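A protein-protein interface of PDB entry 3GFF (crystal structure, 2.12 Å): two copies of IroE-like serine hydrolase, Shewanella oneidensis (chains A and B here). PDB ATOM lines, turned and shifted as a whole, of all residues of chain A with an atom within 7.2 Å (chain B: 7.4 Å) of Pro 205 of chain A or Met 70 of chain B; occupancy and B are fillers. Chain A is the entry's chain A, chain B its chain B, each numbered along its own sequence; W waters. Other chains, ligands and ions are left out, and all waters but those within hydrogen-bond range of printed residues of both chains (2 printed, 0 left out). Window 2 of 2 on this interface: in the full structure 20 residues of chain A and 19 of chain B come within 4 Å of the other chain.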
ATOM      1  N   ASN A 203      19.579  23.083   0.757  1.00  0.00           N
ATOM      2  CA  ASN A 203      20.907  22.554   0.440  1.00  0.00           C
ATOM      3  C   ASN A 203      21.333  22.943  -1.005  1.00  0.00           C
ATOM      4  O   ASN A 203      21.603  22.070  -1.839  1.00  0.00           O
ATOM      5  CB  ASN A 203      20.864  21.028   0.621  1.00  0.00           C
ATOM      6  CG  ASN A 203      22.255  20.367   0.543  1.00  0.00           C
ATOM      7  OD1 ASN A 203      23.264  21.011   0.763  1.00  0.00           O
ATOM      8  ND2 ASN A 203      22.291  19.090   0.199  1.00  0.00           N
ATOM      9  N   ASN A 204      21.363  24.245  -1.313  1.00  0.00           N
ATOM     10  CA  ASN A 204      21.685  24.715  -2.681  1.00  0.00           C
ATOM     11  C   ASN A 204      23.183  24.509  -2.952  1.00  0.00           C
ATOM     12  O   ASN A 204      24.011  24.889  -2.101  1.00  0.00           O
ATOM     13  CB  ASN A 204      21.348  26.190  -2.838  1.00  0.00           C
ATOM     14  CG  ASN A 204      21.161  26.611  -4.294  1.00  0.00           C
ATOM     15  OD1 ASN A 204      20.263  26.121  -4.971  1.00  0.00           O
ATOM     16  ND2 ASN A 204      21.956  27.569  -4.752  1.00  0.00           N
ATOM     17  N   PRO A 205      23.539  23.880  -4.096  1.00  0.00           N
ATOM     18  CA  PRO A 205      24.964  23.668  -4.427  1.00  0.00           C
ATOM     19  C   PRO A 205      25.714  24.935  -4.801  1.00  0.00           C
ATOM     20  O   PRO A 205      26.944  24.934  -4.870  1.00  0.00           O
ATOM     21  CB  PRO A 205      24.903  22.729  -5.632  1.00  0.00           C
ATOM     22  CG  PRO A 205      23.537  23.012  -6.242  1.00  0.00           C
ATOM     23  CD  PRO A 205      22.646  23.302  -5.111  1.00  0.00           C
ATOM     24  N   LEU A 206      24.980  26.016  -5.014  1.00  0.00           N
ATOM     25  CA  LEU A 206      25.581  27.280  -5.385  1.00  0.00           C
ATOM     26  C   LEU A 206      25.382  28.387  -4.378  1.00  0.00           C
ATOM     27  O   LEU A 206      24.363  28.468  -3.688  1.00  0.00           O
ATOM     28  CB  LEU A 206      25.000  27.750  -6.713  1.00  0.00           C
ATOM     29  CG  LEU A 206      25.072  26.856  -7.931  1.00  0.00           C
ATOM     30  CD1 LEU A 206      24.427  27.605  -9.105  1.00  0.00           C
ATOM     31  CD2 LEU A 206      26.526  26.513  -8.204  1.00  0.00           C
ATOM     32  N   SER A 207      26.374  29.269  -4.321  1.00  0.00           N
ATOM     33  CA  SER A 207      26.308  30.445  -3.468  1.00  0.00           C
ATOM     34  C   SER A 207      26.700  31.611  -4.348  1.00  0.00           C
ATOM     35  O   SER A 207      27.792  31.609  -4.960  1.00  0.00           O
ATOM     36  CB  SER A 207      27.240  30.339  -2.275  1.00  0.00           C
ATOM     37  OG  SER A 207      26.883  29.264  -1.432  1.00  0.00           O
ATOM     38  N   PHE A 210      30.189  32.855  -5.668  1.00  0.00           N
ATOM     39  CA  PHE A 210      31.165  31.779  -5.397  1.00  0.00           C
ATOM     40  C   PHE A 210      31.034  30.578  -6.320  1.00  0.00           C
ATOM     41  O   PHE A 210      31.976  29.793  -6.465  1.00  0.00           O
ATOM     42  CB  PHE A 210      31.116  31.322  -3.920  1.00  0.00           C
ATOM     43  CG  PHE A 210      31.570  32.383  -2.925  1.00  0.00           C
ATOM     44  CD1 PHE A 210      32.867  32.901  -2.983  1.00  0.00           C
ATOM     45  CD2 PHE A 210      30.718  32.836  -1.916  1.00  0.00           C
ATOM     46  CE1 PHE A 210      33.289  33.847  -2.080  1.00  0.00           C
ATOM     47  CE2 PHE A 210      31.145  33.775  -1.000  1.00  0.00           C
ATOM     48  CZ  PHE A 210      32.436  34.291  -1.081  1.00  0.00           C
ATOM     49  N   GLY A 211      29.899  30.415  -6.980  1.00  0.00           N
ATOM     50  CA  GLY A 211      29.748  29.255  -7.840  1.00  0.00           C
ATOM     51  C   GLY A 211      29.389  28.096  -6.956  1.00  0.00           C
ATOM     52  O   GLY A 211      28.579  28.261  -6.044  1.00  0.00           O
ATOM     53  N   VAL A 212      29.979  26.943  -7.225  1.00  0.00           N
ATOM     54  CA  VAL A 212      29.747  25.729  -6.452  1.00  0.00           C
ATOM     55  C   VAL A 212      30.371  25.954  -5.090  1.00  0.00           C
ATOM     56  O   VAL A 212      31.600  26.006  -4.938  1.00  0.00           O
ATOM     57  CB  VAL A 212      30.285  24.485  -7.174  1.00  0.00           C
ATOM     58  CG1 VAL A 212      30.154  23.230  -6.318  1.00  0.00           C
ATOM     59  CG2 VAL A 212      29.515  24.316  -8.461  1.00  0.00           C
ATOM     60  N   SER A 213      29.491  26.148  -4.110  1.00  0.00           N
ATOM     61  CA  SER A 213      29.890  26.534  -2.785  1.00  0.00           C
ATOM     62  C   SER A 213      28.701  26.480  -1.832  1.00  0.00           C
ATOM     63  O   SER A 213      27.607  26.915  -2.175  1.00  0.00           O
ATOM     64  CB  SER A 213      30.451  27.963  -2.900  1.00  0.00           C
ATOM     65  OG  SER A 213      30.349  28.713  -1.728  1.00  0.00           O
ATOM     66  N   SER A 214      28.931  26.000  -0.614  1.00  0.00           N
ATOM     67  CA  SER A 214      27.885  25.926   0.397  1.00  0.00           C
ATOM     68  C   SER A 214      27.887  27.135   1.342  1.00  0.00           C
ATOM     69  O   SER A 214      27.253  27.090   2.386  1.00  0.00           O
ATOM     70  CB  SER A 214      28.011  24.606   1.190  1.00  0.00           C
ATOM     71  OG  SER A 214      29.280  24.511   1.789  1.00  0.00           O
ATOM     72  N   TYR A 215      28.553  28.221   0.948  1.00  0.00           N
ATOM     73  CA  TYR A 215      28.667  29.429   1.770  1.00  0.00           C
ATOM     74  C   TYR A 215      27.323  29.973   2.255  1.00  0.00           C
ATOM     75  O   TYR A 215      27.197  30.358   3.406  1.00  0.00           O
ATOM     76  CB  TYR A 215      29.418  30.501   0.971  1.00  0.00           C
ATOM     77  CG  TYR A 215      29.592  31.829   1.669  1.00  0.00           C
ATOM     78  CD1 TYR A 215      30.683  32.052   2.490  1.00  0.00           C
ATOM     79  CD2 TYR A 215      28.698  32.872   1.473  1.00  0.00           C
ATOM     80  CE1 TYR A 215      30.866  33.257   3.121  1.00  0.00           C
ATOM     81  CE2 TYR A 215      28.885  34.106   2.107  1.00  0.00           C
ATOM     82  CZ  TYR A 215      29.976  34.279   2.929  1.00  0.00           C
ATOM     83  OH  TYR A 215      30.226  35.474   3.558  1.00  0.00           O
ATOM     84  N   GLU A 245      16.335  19.755  -0.831  1.00  0.00           N
ATOM     85  CA  GLU A 245      15.760  20.921  -1.440  1.00  0.00           C
ATOM     86  C   GLU A 245      16.841  21.909  -1.893  1.00  0.00           C
ATOM     87  O   GLU A 245      18.006  21.911  -1.401  1.00  0.00           O
ATOM     88  CB  GLU A 245      14.790  21.633  -0.471  1.00  0.00           C
ATOM     89  CG  GLU A 245      13.564  20.784   0.001  1.00  0.00           C
ATOM     90  CD  GLU A 245      12.554  20.492  -1.083  1.00  0.00           C
ATOM     91  OE1 GLU A 245      12.394  21.286  -2.036  1.00  0.00           O
ATOM     92  OE2 GLU A 245      11.890  19.455  -0.970  1.00  0.00           O
ATOM     93  N   THR A 246      16.432  22.740  -2.851  1.00  0.00           N
ATOM     94  CA  THR A 246      17.263  23.782  -3.415  1.00  0.00           C
ATOM     95  C   THR A 246      16.788  25.125  -2.868  1.00  0.00           C
ATOM     96  O   THR A 246      15.746  25.251  -2.214  1.00  0.00           O
ATOM     97  CB  THR A 246      17.151  23.835  -4.934  1.00  0.00           C
ATOM     98  OG1 THR A 246      15.835  24.256  -5.268  1.00  0.00           O
ATOM     99  CG2 THR A 246      17.449  22.480  -5.593  1.00  0.00           C
ATOM    100  N   HIS A 247      17.571  26.151  -3.153  1.00  0.00           N
ATOM    101  CA  HIS A 247      17.264  27.471  -2.673  1.00  0.00           C
ATOM    102  C   HIS A 247      15.891  27.944  -3.166  1.00  0.00           C
ATOM    103  O   HIS A 247      15.068  28.510  -2.424  1.00  0.00           O
ATOM    104  CB  HIS A 247      18.374  28.414  -3.129  1.00  0.00           C
ATOM    105  CG  HIS A 247      18.084  29.839  -2.863  1.00  0.00           C
ATOM    106  ND1 HIS A 247      17.959  30.333  -1.589  1.00  0.00           N
ATOM    107  CD2 HIS A 247      17.915  30.884  -3.701  1.00  0.00           C
ATOM    108  CE1 HIS A 247      17.710  31.628  -1.658  1.00  0.00           C
ATOM    109  NE2 HIS A 247      17.694  31.988  -2.926  1.00  0.00           N
ATOM    110  N   GLN A 248      15.631  27.692  -4.427  1.00  0.00           N
ATOM    111  CA  GLN A 248      14.330  28.043  -4.973  1.00  0.00           C
ATOM    112  C   GLN A 248      13.194  27.064  -4.549  1.00  0.00           C
ATOM    113  O   GLN A 248      12.139  27.528  -4.121  1.00  0.00           O
ATOM    114  CB  GLN A 248      14.431  28.283  -6.493  1.00  0.00           C
ATOM    115  CG  GLN A 248      15.138  29.638  -6.828  1.00  0.00           C
ATOM    116  CD  GLN A 248      14.343  30.875  -6.358  1.00  0.00           C
ATOM    117  OE1 GLN A 248      13.114  30.881  -6.343  1.00  0.00           O
ATOM    118  NE2 GLN A 248      15.054  31.926  -5.985  1.00  0.00           N
ATOM    119  N   SER A 249      13.417  25.747  -4.602  1.00  0.00           N
ATOM    120  CA  SER A 249      12.324  24.772  -4.264  1.00  0.00           C
ATOM    121  C   SER A 249      11.868  24.758  -2.797  1.00  0.00           C
ATOM    122  O   SER A 249      10.803  24.227  -2.483  1.00  0.00           O
ATOM    123  CB  SER A 249      12.704  23.333  -4.624  1.00  0.00           C
ATOM    124  OG  SER A 249      13.505  22.726  -3.613  1.00  0.00           O
ATOM    125  N   PHE B  64       5.280  24.268  -9.951  1.00  0.00           N
ATOM    126  CA  PHE B  64       6.334  24.803  -9.107  1.00  0.00           C
ATOM    127  C   PHE B  64       7.560  23.869  -9.035  1.00  0.00           C
ATOM    128  O   PHE B  64       8.711  24.315  -9.037  1.00  0.00           O
ATOM    129  CB  PHE B  64       5.823  25.012  -7.671  1.00  0.00           C
ATOM    130  CG  PHE B  64       6.911  25.411  -6.696  1.00  0.00           C
ATOM    131  CD1 PHE B  64       7.294  26.729  -6.582  1.00  0.00           C
ATOM    132  CD2 PHE B  64       7.562  24.451  -5.923  1.00  0.00           C
ATOM    133  CE1 PHE B  64       8.312  27.097  -5.712  1.00  0.00           C
ATOM    134  CE2 PHE B  64       8.570  24.807  -5.038  1.00  0.00           C
ATOM    135  CZ  PHE B  64       8.944  26.136  -4.929  1.00  0.00           C
ATOM    136  N   LEU B  65       7.301  22.583  -8.897  1.00  0.00           N
ATOM    137  CA  LEU B  65       8.365  21.591  -8.767  1.00  0.00           C
ATOM    138  C   LEU B  65       9.169  21.466 -10.065  1.00  0.00           C
ATOM    139  O   LEU B  65      10.306  21.079 -10.017  1.00  0.00           O
ATOM    140  CB  LEU B  65       7.806  20.210  -8.398  1.00  0.00           C
ATOM    141  CG  LEU B  65       7.248  19.942  -6.986  1.00  0.00           C
ATOM    142  CD1 LEU B  65       6.482  18.674  -6.888  1.00  0.00           C
ATOM    143  CD2 LEU B  65       8.366  19.970  -5.973  1.00  0.00           C
ATOM    144  N   SER B  66       8.581  21.817 -11.209  1.00  0.00           N
ATOM    145  CA  SER B  66       9.252  21.651 -12.506  1.00  0.00           C
ATOM    146  C   SER B  66       9.843  22.924 -13.072  1.00  0.00           C
ATOM    147  O   SER B  66      10.424  22.912 -14.160  1.00  0.00           O
ATOM    148  CB  SER B  66       8.258  21.089 -13.517  1.00  0.00           C
ATOM    149  OG  SER B  66       7.219  22.006 -13.769  1.00  0.00           O
ATOM    150  N   GLN B  67       9.718  24.027 -12.348  1.00  0.00           N
ATOM    151  CA  GLN B  67      10.193  25.314 -12.861  1.00  0.00           C
ATOM    152  C   GLN B  67      11.567  25.633 -12.275  1.00  0.00           C
ATOM    153  O   GLN B  67      12.008  24.980 -11.339  1.00  0.00           O
ATOM    154  CB  GLN B  67       9.190  26.435 -12.530  1.00  0.00           C
ATOM    155  CG  GLN B  67       9.175  26.816 -11.056  1.00  0.00           C
ATOM    156  CD  GLN B  67       8.191  27.930 -10.748  1.00  0.00           C
ATOM    157  OE1 GLN B  67       7.311  28.208 -11.547  1.00  0.00           O
ATOM    158  NE2 GLN B  67       8.354  28.579  -9.600  1.00  0.00           N
ATOM    159  N   GLY B  68      12.236  26.633 -12.839  1.00  0.00           N
ATOM    160  CA  GLY B  68      13.526  27.074 -12.326  1.00  0.00           C
ATOM    161  C   GLY B  68      14.730  26.457 -13.033  1.00  0.00           C
ATOM    162  O   GLY B  68      14.588  25.774 -14.058  1.00  0.00           O
ATOM    163  N   THR B  69      15.909  26.727 -12.479  1.00  0.00           N
ATOM    164  CA  THR B  69      17.170  26.236 -13.016  1.00  0.00           C
ATOM    165  C   THR B  69      17.519  24.833 -12.511  1.00  0.00           C
ATOM    166  O   THR B  69      18.342  24.136 -13.124  1.00  0.00           O
ATOM    167  CB  THR B  69      18.318  27.186 -12.651  1.00  0.00           C
ATOM    168  OG1 THR B  69      18.441  27.281 -11.221  1.00  0.00           O
ATOM    169  CG2 THR B  69      18.072  28.573 -13.245  1.00  0.00           C
ATOM    170  N   MET B  70      16.895  24.418 -11.412  1.00  0.00           N
ATOM    171  CA  MET B  70      17.162  23.117 -10.812  1.00  0.00           C
ATOM    172  C   MET B  70      15.846  22.407 -10.560  1.00  0.00           C
ATOM    173  O   MET B  70      15.549  22.031  -9.418  1.00  0.00           O
ATOM    174  CB  MET B  70      17.893  23.292  -9.477  1.00  0.00           C
ATOM    175  CG  MET B  70      19.048  24.256  -9.547  1.00  0.00           C
ATOM    176  SD  MET B  70      19.790  24.515  -7.802  1.00  0.00           S
ATOM    177  CE  MET B  70      20.519  22.568  -7.598  1.00  0.00           C
ATOM    178  N   PRO B  71      15.081  22.149 -11.634  1.00  0.00           N
ATOM    179  CA  PRO B  71      13.788  21.547 -11.462  1.00  0.00           C
ATOM    180  C   PRO B  71      13.889  20.222 -10.701  1.00  0.00           C
ATOM    181  O   PRO B  71      14.830  19.451 -10.885  1.00  0.00           O
ATOM    182  CB  PRO B  71      13.293  21.337 -12.901  1.00  0.00           C
ATOM    183  CG  PRO B  71      14.490  21.402 -13.751  1.00  0.00           C
ATOM    184  CD  PRO B  71      15.404  22.343 -13.056  1.00  0.00           C
ATOM    185  N   GLN B  72      12.883  19.962  -9.874  1.00  0.00           N
ATOM    186  CA  GLN B  72      12.871  18.800  -8.996  1.00  0.00           C
ATOM    187  C   GLN B  72      12.153  17.642  -9.653  1.00  0.00           C
ATOM    188  O   GLN B  72      12.312  16.501  -9.253  1.00  0.00           O
ATOM    189  CB  GLN B  72      12.239  19.209  -7.663  1.00  0.00           C
ATOM    190  CG  GLN B  72      13.028  20.332  -6.999  1.00  0.00           C
ATOM    191  CD  GLN B  72      14.390  19.862  -6.547  1.00  0.00           C
ATOM    192  OE1 GLN B  72      14.512  19.080  -5.599  1.00  0.00           O
ATOM    193  NE2 GLN B  72      15.427  20.333  -7.228  1.00  0.00           N
ATOM    194  N   ILE B  73      11.317  17.959 -10.632  1.00  0.00           N
ATOM    195  CA  ILE B  73      10.680  16.933 -11.432  1.00  0.00           C
ATOM    196  C   ILE B  73      10.743  17.493 -12.842  1.00  0.00           C
ATOM    197  O   ILE B  73      11.037  18.665 -13.011  1.00  0.00           O
ATOM    198  CB  ILE B  73       9.237  16.580 -10.999  1.00  0.00           C
ATOM    199  CG1 ILE B  73       8.284  17.774 -11.165  1.00  0.00           C
ATOM    200  CG2 ILE B  73       9.217  15.980  -9.553  1.00  0.00           C
ATOM    201  CD1 ILE B  73       6.807  17.419 -10.969  1.00  0.00           C
ATOM    202  N   ASP B 269      23.150  15.643 -11.975  1.00  0.00           N
ATOM    203  CA  ASP B 269      23.986  16.496 -11.145  1.00  0.00           C
ATOM    204  C   ASP B 269      25.302  16.842 -11.855  1.00  0.00           C
ATOM    205  O   ASP B 269      26.225  16.027 -11.927  1.00  0.00           O
ATOM    206  CB  ASP B 269      24.273  15.812  -9.816  1.00  0.00           C
ATOM    207  CG  ASP B 269      25.147  16.652  -8.908  1.00  0.00           C
ATOM    208  OD1 ASP B 269      25.302  17.864  -9.195  1.00  0.00           O
ATOM    209  OD2 ASP B 269      25.691  16.105  -7.912  1.00  0.00           O
ATOM    210  N   TYR B 271      27.806  18.085 -10.876  1.00  0.00           N
ATOM    211  CA  TYR B 271      28.985  18.005  -9.972  1.00  0.00           C
ATOM    212  C   TYR B 271      29.209  16.558  -9.481  1.00  0.00           C
ATOM    213  O   TYR B 271      30.067  15.829 -10.016  1.00  0.00           O
ATOM    214  CB  TYR B 271      28.824  18.960  -8.777  1.00  0.00           C
ATOM    215  CG  TYR B 271      27.989  20.162  -9.136  1.00  0.00           C
ATOM    216  CD1 TYR B 271      28.459  21.122 -10.031  1.00  0.00           C
ATOM    217  CD2 TYR B 271      26.709  20.324  -8.607  1.00  0.00           C
ATOM    218  CE1 TYR B 271      27.664  22.223 -10.389  1.00  0.00           C
ATOM    219  CE2 TYR B 271      25.912  21.407  -8.949  1.00  0.00           C
ATOM    220  CZ  TYR B 271      26.387  22.360  -9.836  1.00  0.00           C
ATOM    221  OH  TYR B 271      25.580  23.432 -10.181  1.00  0.00           O
ATOM    222  N   TYR B 301      15.798  20.660 -20.244  1.00  0.00           N
ATOM    223  CA  TYR B 301      16.650  20.410 -19.104  1.00  0.00           C
ATOM    224  C   TYR B 301      18.111  20.406 -19.528  1.00  0.00           C
ATOM    225  O   TYR B 301      18.922  21.126 -18.939  1.00  0.00           O
ATOM    226  CB  TYR B 301      16.187  19.116 -18.428  1.00  0.00           C
ATOM    227  CG  TYR B 301      16.949  18.724 -17.209  1.00  0.00           C
ATOM    228  CD1 TYR B 301      17.161  19.622 -16.179  1.00  0.00           C
ATOM    229  CD2 TYR B 301      17.412  17.433 -17.057  1.00  0.00           C
ATOM    230  CE1 TYR B 301      17.862  19.249 -15.043  1.00  0.00           C
ATOM    231  CE2 TYR B 301      18.119  17.049 -15.929  1.00  0.00           C
ATOM    232  CZ  TYR B 301      18.341  17.952 -14.935  1.00  0.00           C
ATOM    233  OH  TYR B 301      19.037  17.549 -13.836  1.00  0.00           O
ATOM    234  N   GLN B 304      19.383  23.986 -20.371  1.00  0.00           N
ATOM    235  CA  GLN B 304      19.691  24.740 -19.183  1.00  0.00           C
ATOM    236  C   GLN B 304      21.063  24.339 -18.670  1.00  0.00           C
ATOM    237  O   GLN B 304      21.941  25.186 -18.509  1.00  0.00           O
ATOM    238  CB  GLN B 304      18.666  24.447 -18.110  1.00  0.00           C
ATOM    239  CG  GLN B 304      17.326  25.022 -18.387  1.00  0.00           C
ATOM    240  CD  GLN B 304      16.585  25.226 -17.096  1.00  0.00           C
ATOM    241  OE1 GLN B 304      16.404  24.277 -16.321  1.00  0.00           O
ATOM    242  NE2 GLN B 304      16.192  26.481 -16.824  1.00  0.00           N
ATOM    243  N   LEU B 305      21.245  23.043 -18.424  1.00  0.00           N
ATOM    244  CA  LEU B 305      22.538  22.530 -17.959  1.00  0.00           C
ATOM    245  C   LEU B 305      23.670  23.105 -18.833  1.00  0.00           C
ATOM    246  O   LEU B 305      24.672  23.609 -18.307  1.00  0.00           O
ATOM    247  CB  LEU B 305      22.555  20.994 -17.936  1.00  0.00           C
ATOM    248  CG  LEU B 305      21.535  20.287 -17.020  1.00  0.00           C
ATOM    249  CD1 LEU B 305      21.510  18.740 -17.230  1.00  0.00           C
ATOM    250  CD2 LEU B 305      21.755  20.633 -15.540  1.00  0.00           C
HETATM  251  O   HOH W   1      17.773  27.017  -6.581  1.00  0.00           O
HETATM  252  O   HOH W   2      14.370  23.826  -7.553  1.00  0.00           O
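The side-chain amide oxygen (OD1) of Asn 204 of chain A lies close to the side-chain sulfur (SD) of Met 70 of chain B (3.3 Å).
The backbone carbonyl oxygen (O) of Leu 206 of chain A is in hydrogen-bond range of the side-chain amide nitrogen (ND2) of Asn 204 of chain A (2.8 Å). N of Tyr 271 of chain B sits close to OD1 of Asp 269 of chain B (3.0 Å). The backbone NH (N) of Ser 249 of chain A sits at hydrogen-bond distance from the side-chain hydroxyl (OG1) of Thr 246 of chain A. N of Ser 213 of chain A is in hydrogen-bond range of O of Pro 205 of chain A, 2.9 Å away. O of Leu 65 of chain B sits at hydrogen-bond distance from N of Gln 72 of chain B, 2.8 Å away. The side-chain carboxylate (OE1) of Glu 245 of chain A lies within hydrogen-bond range of the side-chain hydroxyl (OG) of Ser 249 of chain A (2.4 Å).
CE of Met 70 of chain B touches CG of Pro 205 of chain A (3.3 Å). Pro 205 of chain A touches Tyr 271 of chain B (CB to CE2, 3.7 Å). Tyr 271 of chain B touches Leu 206 of chain A. Val 212 of chain A touches Tyr 271 of chain B (CG2 to CE1, 3.4 Å). Met 70 of chain B touches Thr 246 of chain A (CE to CG2, 3.7 Å). NE2 of Gln 72 of chain B touches CG2 of Thr 246 of chain A (3.4 Å). Phe 64 of chain B touches Gln 248 of chain A (CZ to O, 3.6 Å). CE2 of Phe 64 of chain B touches O of Ser 249 of chain A (3.4 Å). CG of Gln 72 of chain B touches CB of Ser 249 of chain A (3.8 Å).
Met 70 of chain B touches just these residues of chain A: Asn 204 (3.3 Å), Pro 205 (3.3 Å) and Thr 246 (3.7 Å). Of the printed residues of chain B, Thr 246 of chain A touches Met 70 (3.7 Å) and Gln 72 (3.4 Å). Of the printed residues of chain A, Phe 64 of chain B touches Gln 248 (3.6 Å) and Ser 249 (3.4 Å). Tyr 215 of chain A touches none of the printed residues of chain B. Asn 203 of chain A touches none of the printed residues of chain B. The nearest residue of chain B that does not touch Pro 205 of chain A is Asp 269 of chain B (6.0 Å). The nearest printed residue of chain B that does not touch Leu 206 of chain A is Met 70 of chain B (5.7 Å).
Among the printed residues, no Asp or Glu carboxylate lies within 4 Å of a Lys or Arg side-chain nitrogen of the other chain.
No position is printed for both chains. Of the 10 pairs that touch across the chains among the printed residues, none has its exchanged pair printed and touching as well.
Water W2 lies within hydrogen-bond range of OG1 of Thr 246 of chain A and O of Met 70 of chain B. Water W1 lies within hydrogen-bond range of OD1 of Asn 204 of chain A (3.1 Å), N of Gln 248 of chain A (3.1 Å) and SD of Met 70 of chain B (3.4 Å).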
